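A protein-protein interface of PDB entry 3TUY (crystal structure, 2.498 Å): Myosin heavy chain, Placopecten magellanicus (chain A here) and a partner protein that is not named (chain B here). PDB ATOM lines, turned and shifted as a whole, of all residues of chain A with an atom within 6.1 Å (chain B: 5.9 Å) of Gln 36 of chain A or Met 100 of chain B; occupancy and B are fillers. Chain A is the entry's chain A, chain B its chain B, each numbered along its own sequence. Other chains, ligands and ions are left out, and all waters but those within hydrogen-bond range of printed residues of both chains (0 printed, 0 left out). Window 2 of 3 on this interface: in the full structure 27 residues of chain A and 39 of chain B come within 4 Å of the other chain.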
ATOM      1  N   LYS A  31       0.123  -2.362   7.151  1.00  0.00           N
ATOM      2  CA  LYS A  31       1.493  -1.971   7.436  1.00  0.00           C
ATOM      3  C   LYS A  31       1.610  -0.563   8.057  1.00  0.00           C
ATOM      4  O   LYS A  31       2.374  -0.349   9.001  1.00  0.00           O
ATOM      5  CB  LYS A  31       2.322  -2.094   6.164  1.00  0.00           C
ATOM      6  CG  LYS A  31       3.427  -1.076   6.011  1.00  0.00           C
ATOM      7  CD  LYS A  31       4.678  -1.468   6.768  1.00  0.00           C
ATOM      8  CE  LYS A  31       5.829  -0.562   6.334  1.00  0.00           C
ATOM      9  NZ  LYS A  31       7.046  -0.689   7.202  1.00  0.00           N
ATOM     10  N   LYS A  32       0.846   0.386   7.535  1.00  0.00           N
ATOM     11  CA  LYS A  32       0.843   1.727   8.085  1.00  0.00           C
ATOM     12  C   LYS A  32       0.193   1.719   9.471  1.00  0.00           C
ATOM     13  O   LYS A  32       0.567   2.492  10.356  1.00  0.00           O
ATOM     14  CB  LYS A  32       0.113   2.682   7.144  1.00  0.00           C
ATOM     15  CG  LYS A  32      -0.207   4.035   7.721  1.00  0.00           C
ATOM     16  CD  LYS A  32      -1.374   4.695   6.953  1.00  0.00           C
ATOM     17  CE  LYS A  32      -1.373   6.238   7.095  1.00  0.00           C
ATOM     18  NZ  LYS A  32      -2.658   6.892   6.660  1.00  0.00           N
ATOM     19  N   LEU A  33      -0.780   0.842   9.664  1.00  0.00           N
ATOM     20  CA  LEU A  33      -1.423   0.745  10.960  1.00  0.00           C
ATOM     21  C   LEU A  33      -0.420   0.267  12.012  1.00  0.00           C
ATOM     22  O   LEU A  33      -0.433   0.731  13.150  1.00  0.00           O
ATOM     23  CB  LEU A  33      -2.602  -0.216  10.895  1.00  0.00           C
ATOM     24  CG  LEU A  33      -3.705   0.028  11.924  1.00  0.00           C
ATOM     25  CD1 LEU A  33      -4.339   1.434  11.745  1.00  0.00           C
ATOM     26  CD2 LEU A  33      -4.738  -1.084  11.822  1.00  0.00           C
ATOM     27  N   GLN A  34       0.451  -0.657  11.625  1.00  0.00           N
ATOM     28  CA  GLN A  34       1.472  -1.137  12.536  1.00  0.00           C
ATOM     29  C   GLN A  34       2.504  -0.063  12.850  1.00  0.00           C
ATOM     30  O   GLN A  34       2.838   0.165  14.023  1.00  0.00           O
ATOM     31  CB  GLN A  34       2.166  -2.367  11.978  1.00  0.00           C
ATOM     32  CG  GLN A  34       1.328  -3.609  12.081  1.00  0.00           C
ATOM     33  CD  GLN A  34       2.102  -4.861  11.673  1.00  0.00           C
ATOM     34  OE1 GLN A  34       1.913  -5.944  12.261  1.00  0.00           O
ATOM     35  NE2 GLN A  34       2.984  -4.722  10.664  1.00  0.00           N
ATOM     36  N   ASP A  35       3.025   0.586  11.811  1.00  0.00           N
ATOM     37  CA  ASP A  35       3.980   1.659  12.020  1.00  0.00           C
ATOM     38  C   ASP A  35       3.398   2.741  12.910  1.00  0.00           C
ATOM     39  O   ASP A  35       4.048   3.196  13.828  1.00  0.00           O
ATOM     40  CB  ASP A  35       4.437   2.269  10.704  1.00  0.00           C
ATOM     41  CG  ASP A  35       5.293   1.321   9.883  1.00  0.00           C
ATOM     42  OD1 ASP A  35       5.735   0.275  10.415  1.00  0.00           O
ATOM     43  OD2 ASP A  35       5.523   1.640   8.698  1.00  0.00           O
ATOM     44  N   GLN A  36       2.172   3.151  12.641  1.00  0.00           N
ATOM     45  CA  GLN A  36       1.517   4.148  13.465  1.00  0.00           C
ATOM     46  C   GLN A  36       1.373   3.718  14.921  1.00  0.00           C
ATOM     47  O   GLN A  36       1.430   4.551  15.822  1.00  0.00           O
ATOM     48  CB  GLN A  36       0.163   4.486  12.883  1.00  0.00           C
ATOM     49  CG  GLN A  36       0.270   5.409  11.701  1.00  0.00           C
ATOM     50  CD  GLN A  36      -1.049   5.603  11.018  1.00  0.00           C
ATOM     51  OE1 GLN A  36      -1.929   4.766  11.117  1.00  0.00           O
ATOM     52  NE2 GLN A  36      -1.201   6.710  10.332  1.00  0.00           N
ATOM     53  N   ARG A  37       1.177   2.418  15.145  1.00  0.00           N
ATOM     54  CA  ARG A  37       1.092   1.889  16.492  1.00  0.00           C
ATOM     55  C   ARG A  37       2.386   2.190  17.226  1.00  0.00           C
ATOM     56  O   ARG A  37       2.363   2.687  18.357  1.00  0.00           O
ATOM     57  CB  ARG A  37       0.836   0.380  16.481  1.00  0.00           C
ATOM     58  CG  ARG A  37       0.612  -0.232  17.867  1.00  0.00           C
ATOM     59  CD  ARG A  37       1.581  -1.367  18.132  1.00  0.00           C
ATOM     60  NE  ARG A  37       0.916  -2.590  18.598  1.00  0.00           N
ATOM     61  CZ  ARG A  37       1.024  -3.784  18.003  1.00  0.00           C
ATOM     62  NH1 ARG A  37       1.763  -3.925  16.908  1.00  0.00           N
ATOM     63  NH2 ARG A  37       0.391  -4.844  18.496  1.00  0.00           N
ATOM     64  N   ILE A  38       3.512   1.887  16.580  1.00  0.00           N
ATOM     65  CA  ILE A  38       4.827   2.230  17.121  1.00  0.00           C
ATOM     66  C   ILE A  38       4.979   3.733  17.319  1.00  0.00           C
ATOM     67  O   ILE A  38       5.367   4.182  18.399  1.00  0.00           O
ATOM     68  CB  ILE A  38       5.966   1.746  16.222  1.00  0.00           C
ATOM     69  CG1 ILE A  38       6.124   0.243  16.325  1.00  0.00           C
ATOM     70  CG2 ILE A  38       7.287   2.368  16.630  1.00  0.00           C
ATOM     71  CD1 ILE A  38       6.584  -0.353  15.027  1.00  0.00           C
ATOM     72  N   GLY A  39       4.702   4.506  16.270  1.00  0.00           N
ATOM     73  CA  GLY A  39       4.757   5.954  16.352  1.00  0.00           C
ATOM     74  C   GLY A  39       3.999   6.483  17.565  1.00  0.00           C
ATOM     75  O   GLY A  39       4.546   7.256  18.342  1.00  0.00           O
ATOM     76  N   LEU A  40       2.756   6.047  17.748  1.00  0.00           N
ATOM     77  CA  LEU A  40       1.942   6.550  18.843  1.00  0.00           C
ATOM     78  C   LEU A  40       2.454   6.098  20.218  1.00  0.00           C
ATOM     79  O   LEU A  40       2.255   6.787  21.224  1.00  0.00           O
ATOM     80  CB  LEU A  40       0.479   6.167  18.675  1.00  0.00           C
ATOM     81  CG  LEU A  40      -0.311   6.849  19.792  1.00  0.00           C
ATOM     82  CD1 LEU A  40      -0.208   8.370  19.636  1.00  0.00           C
ATOM     83  CD2 LEU A  40      -1.764   6.391  19.867  1.00  0.00           C
ATOM     84  N   SER A  41       3.112   4.945  20.269  1.00  0.00           N
ATOM     85  CA  SER A  41       3.790   4.540  21.486  1.00  0.00           C
ATOM     86  C   SER A  41       4.963   5.471  21.790  1.00  0.00           C
ATOM     87  O   SER A  41       5.119   5.918  22.930  1.00  0.00           O
ATOM     88  CB  SER A  41       4.269   3.105  21.384  1.00  0.00           C
ATOM     89  OG  SER A  41       3.161   2.278  21.168  1.00  0.00           O
ATOM     90  N   ARG B  95      10.035  13.047  16.039  1.00  0.00           N
ATOM     91  CA  ARG B  95       9.473  13.798  14.915  1.00  0.00           C
ATOM     92  C   ARG B  95       8.962  12.869  13.809  1.00  0.00           C
ATOM     93  O   ARG B  95       7.928  13.133  13.169  1.00  0.00           O
ATOM     94  CB  ARG B  95      10.490  14.766  14.331  1.00  0.00           C
ATOM     95  CG  ARG B  95      10.746  15.971  15.187  1.00  0.00           C
ATOM     96  CD  ARG B  95      11.530  17.013  14.410  1.00  0.00           C
ATOM     97  NE  ARG B  95      12.960  16.800  14.571  1.00  0.00           N
ATOM     98  CZ  ARG B  95      13.737  16.223  13.663  1.00  0.00           C
ATOM     99  NH1 ARG B  95      13.219  15.811  12.499  1.00  0.00           N
ATOM    100  NH2 ARG B  95      15.035  16.081  13.918  1.00  0.00           N
ATOM    101  N   ASN B  96       9.689  11.786  13.577  1.00  0.00           N
ATOM    102  CA  ASN B  96       9.209  10.816  12.615  1.00  0.00           C
ATOM    103  C   ASN B  96       8.002  10.030  13.134  1.00  0.00           C
ATOM    104  O   ASN B  96       7.205   9.513  12.339  1.00  0.00           O
ATOM    105  CB  ASN B  96      10.338   9.900  12.144  1.00  0.00           C
ATOM    106  CG  ASN B  96      11.511  10.684  11.551  1.00  0.00           C
ATOM    107  OD1 ASN B  96      12.671  10.287  11.704  1.00  0.00           O
ATOM    108  ND2 ASN B  96      11.212  11.814  10.889  1.00  0.00           N
ATOM    109  N   ALA B  97       7.863   9.945  14.458  1.00  0.00           N
ATOM    110  CA  ALA B  97       6.683   9.321  15.041  1.00  0.00           C
ATOM    111  C   ALA B  97       5.488  10.202  14.712  1.00  0.00           C
ATOM    112  O   ALA B  97       4.445   9.705  14.327  1.00  0.00           O
ATOM    113  CB  ALA B  97       6.827   9.134  16.584  1.00  0.00           C
ATOM    114  N   PHE B  98       5.643  11.517  14.872  1.00  0.00           N
ATOM    115  CA  PHE B  98       4.599  12.446  14.465  1.00  0.00           C
ATOM    116  C   PHE B  98       4.391  12.383  12.934  1.00  0.00           C
ATOM    117  O   PHE B  98       3.255  12.389  12.459  1.00  0.00           O
ATOM    118  CB  PHE B  98       4.907  13.874  14.918  1.00  0.00           C
ATOM    119  CG  PHE B  98       4.633  14.128  16.379  1.00  0.00           C
ATOM    120  CD1 PHE B  98       3.332  14.311  16.834  1.00  0.00           C
ATOM    121  CD2 PHE B  98       5.669  14.220  17.296  1.00  0.00           C
ATOM    122  CE1 PHE B  98       3.062  14.562  18.175  1.00  0.00           C
ATOM    123  CE2 PHE B  98       5.407  14.468  18.640  1.00  0.00           C
ATOM    124  CZ  PHE B  98       4.100  14.640  19.082  1.00  0.00           C
ATOM    125  N   GLY B  99       5.485  12.306  12.172  1.00  0.00           N
ATOM    126  CA  GLY B  99       5.415  12.278  10.711  1.00  0.00           C
ATOM    127  C   GLY B  99       4.480  11.175  10.228  1.00  0.00           C
ATOM    128  O   GLY B  99       3.757  11.328   9.258  1.00  0.00           O
ATOM    129  N   MET B 100       4.509  10.060  10.943  1.00  0.00           N
ATOM    130  CA  MET B 100       3.618   8.924  10.760  1.00  0.00           C
ATOM    131  C   MET B 100       2.145   9.297  10.549  1.00  0.00           C
ATOM    132  O   MET B 100       1.392   8.545   9.932  1.00  0.00           O
ATOM    133  CB  MET B 100       3.704   8.068  12.023  1.00  0.00           C
ATOM    134  CG  MET B 100       3.759   6.612  11.813  1.00  0.00           C
ATOM    135  SD  MET B 100       5.385   6.232  11.213  1.00  0.00           S
ATOM    136  CE  MET B 100       6.133   5.511  12.692  1.00  0.00           C
ATOM    137  N   PHE B 101       1.724  10.433  11.098  1.00  0.00           N
ATOM    138  CA  PHE B 101       0.320  10.847  11.024  1.00  0.00           C
ATOM    139  C   PHE B 101       0.217  12.119  10.185  1.00  0.00           C
ATOM    140  O   PHE B 101      -0.815  12.791  10.160  1.00  0.00           O
ATOM    141  CB  PHE B 101      -0.257  11.060  12.432  1.00  0.00           C
ATOM    142  CG  PHE B 101      -0.118   9.854  13.329  1.00  0.00           C
ATOM    143  CD1 PHE B 101       0.972   9.725  14.182  1.00  0.00           C
ATOM    144  CD2 PHE B 101      -1.069   8.841  13.309  1.00  0.00           C
ATOM    145  CE1 PHE B 101       1.107   8.599  15.008  1.00  0.00           C
ATOM    146  CE2 PHE B 101      -0.946   7.712  14.125  1.00  0.00           C
ATOM    147  CZ  PHE B 101       0.147   7.591  14.973  1.00  0.00           C
ATOM    148  N   ASP B 102       1.308  12.438   9.497  1.00  0.00           N
ATOM    149  CA  ASP B 102       1.397  13.618   8.652  1.00  0.00           C
ATOM    150  C   ASP B 102       1.813  13.171   7.241  1.00  0.00           C
ATOM    151  O   ASP B 102       2.965  13.357   6.830  1.00  0.00           O
ATOM    152  CB  ASP B 102       2.421  14.587   9.240  1.00  0.00           C
ATOM    153  CG  ASP B 102       2.557  15.875   8.433  1.00  0.00           C
ATOM    154  OD1 ASP B 102       1.581  16.261   7.743  1.00  0.00           O
ATOM    155  OD2 ASP B 102       3.640  16.505   8.505  1.00  0.00           O
ATOM    156  N   GLU B 103       0.874  12.573   6.514  1.00  0.00           N
ATOM    157  CA  GLU B 103       1.177  11.980   5.212  1.00  0.00           C
ATOM    158  C   GLU B 103       1.793  12.975   4.223  1.00  0.00           C
ATOM    159  O   GLU B 103       2.792  12.668   3.559  1.00  0.00           O
ATOM    160  CB  GLU B 103      -0.072  11.324   4.619  1.00  0.00           C
ATOM    161  CG  GLU B 103      -0.119   9.804   4.795  1.00  0.00           C
ATOM    162  CD  GLU B 103       0.749   9.061   3.773  1.00  0.00           C
ATOM    163  OE1 GLU B 103       0.182   8.461   2.825  1.00  0.00           O
ATOM    164  OE2 GLU B 103       1.998   9.075   3.912  1.00  0.00           O
ATOM    165  N   TYR B 113      -7.155  15.948  15.750  1.00  0.00           N
ATOM    166  CA  TYR B 113      -6.577  14.650  15.418  1.00  0.00           C
ATOM    167  C   TYR B 113      -5.620  14.155  16.507  1.00  0.00           C
ATOM    168  O   TYR B 113      -5.827  13.098  17.092  1.00  0.00           O
ATOM    169  CB  TYR B 113      -5.829  14.774  14.089  1.00  0.00           C
ATOM    170  CG  TYR B 113      -5.352  13.465  13.495  1.00  0.00           C
ATOM    171  CD1 TYR B 113      -5.982  12.272  13.819  1.00  0.00           C
ATOM    172  CD2 TYR B 113      -4.277  13.432  12.601  1.00  0.00           C
ATOM    173  CE1 TYR B 113      -5.567  11.071  13.267  1.00  0.00           C
ATOM    174  CE2 TYR B 113      -3.835  12.229  12.051  1.00  0.00           C
ATOM    175  CZ  TYR B 113      -4.492  11.048  12.393  1.00  0.00           C
ATOM    176  OH  TYR B 113      -4.104   9.828  11.878  1.00  0.00           O
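The side-chain carboxylate of Asp 35 of chain A lies within salt-bridge range of the side-chain amino group of Lys 31 of chain A (3.2 Å). The backbone carbonyl oxygen (O) of Lys 32 of chain A lies close to the side-chain amide oxygen (OE1) of Gln 36 of chain A, at 3.5 Å.
The side-chain amide nitrogen (NE2) of Gln 36 of chain A sits at hydrogen-bond distance from the backbone carbonyl oxygen (O) of Met 100 of chain B (3.2 Å).
Of the 10 printed residues of chain B, 3 touch a printed residue of chain A. Hydrophobic or aromatic side chains of chain B that line the printed part of chain A: Ala 97, Met 100 and Phe 101. Printed residues of chain A that touch a printed residue of chain B: Asp 35, Gln 36, Gly 39 and Leu 40. Hydrophobic or aromatic side chains of chain A within 4 Å of the printed part of chain B: Leu 40. Among the printed residues, 6 pairs touch across the chains. Among the printed residues, no Asp or Glu carboxylate lies within 4 Å of a Lys or Arg side-chain nitrogen of the other chain.
Of the printed residues of chain B, Gln 36 of chain A touches Met 100 (3.2 Å) and Phe 101 (3.4 Å). Of the printed residues of chain B, Gly 39 of chain A touches Ala 97 and Met 100. Of the printed residues of chain B, Leu 40 of chain A touches Phe 101 (3.98 Å). Of the printed residues of chain A, Ala 97 of chain B touches Gly 39 (3.4 Å). Of chain A, only Asp 35 (3.3 Å), Gln 36 (3.2 Å) and Gly 39 (3.9 Å) come within 4 Å of Met 100 of chain B. Of the printed residues of chain A, Phe 101 of chain B touches Gln 36 (3.4 Å) and Leu 40 (3.98 Å). The nearest residue of chain B that does not touch Gln 36 of chain A is Tyr 113 of chain B (4.5 Å). The nearest residue of chain A that does not touch Met 100 of chain B is Lys 32 of chain A (4.6 Å). The nearest printed residue of chain A that does not touch Phe 101 of chain B is Gly 39 of chain A (4.4 Å).
Among the printed residues, merely in contact across the chains: Asp 35 of chain A with Met 100 of chain B (3.3 Å), Gln 36 of chain A with Phe 101 of chain B (3.4 Å), Gly 39 of chain A with Ala 97 of chain B (3.4 Å), Gly 39 of chain A with Met 100 of chain B (3.9 Å) and Leu 40 of chain A with Phe 101 of chain B (3.98 Å).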
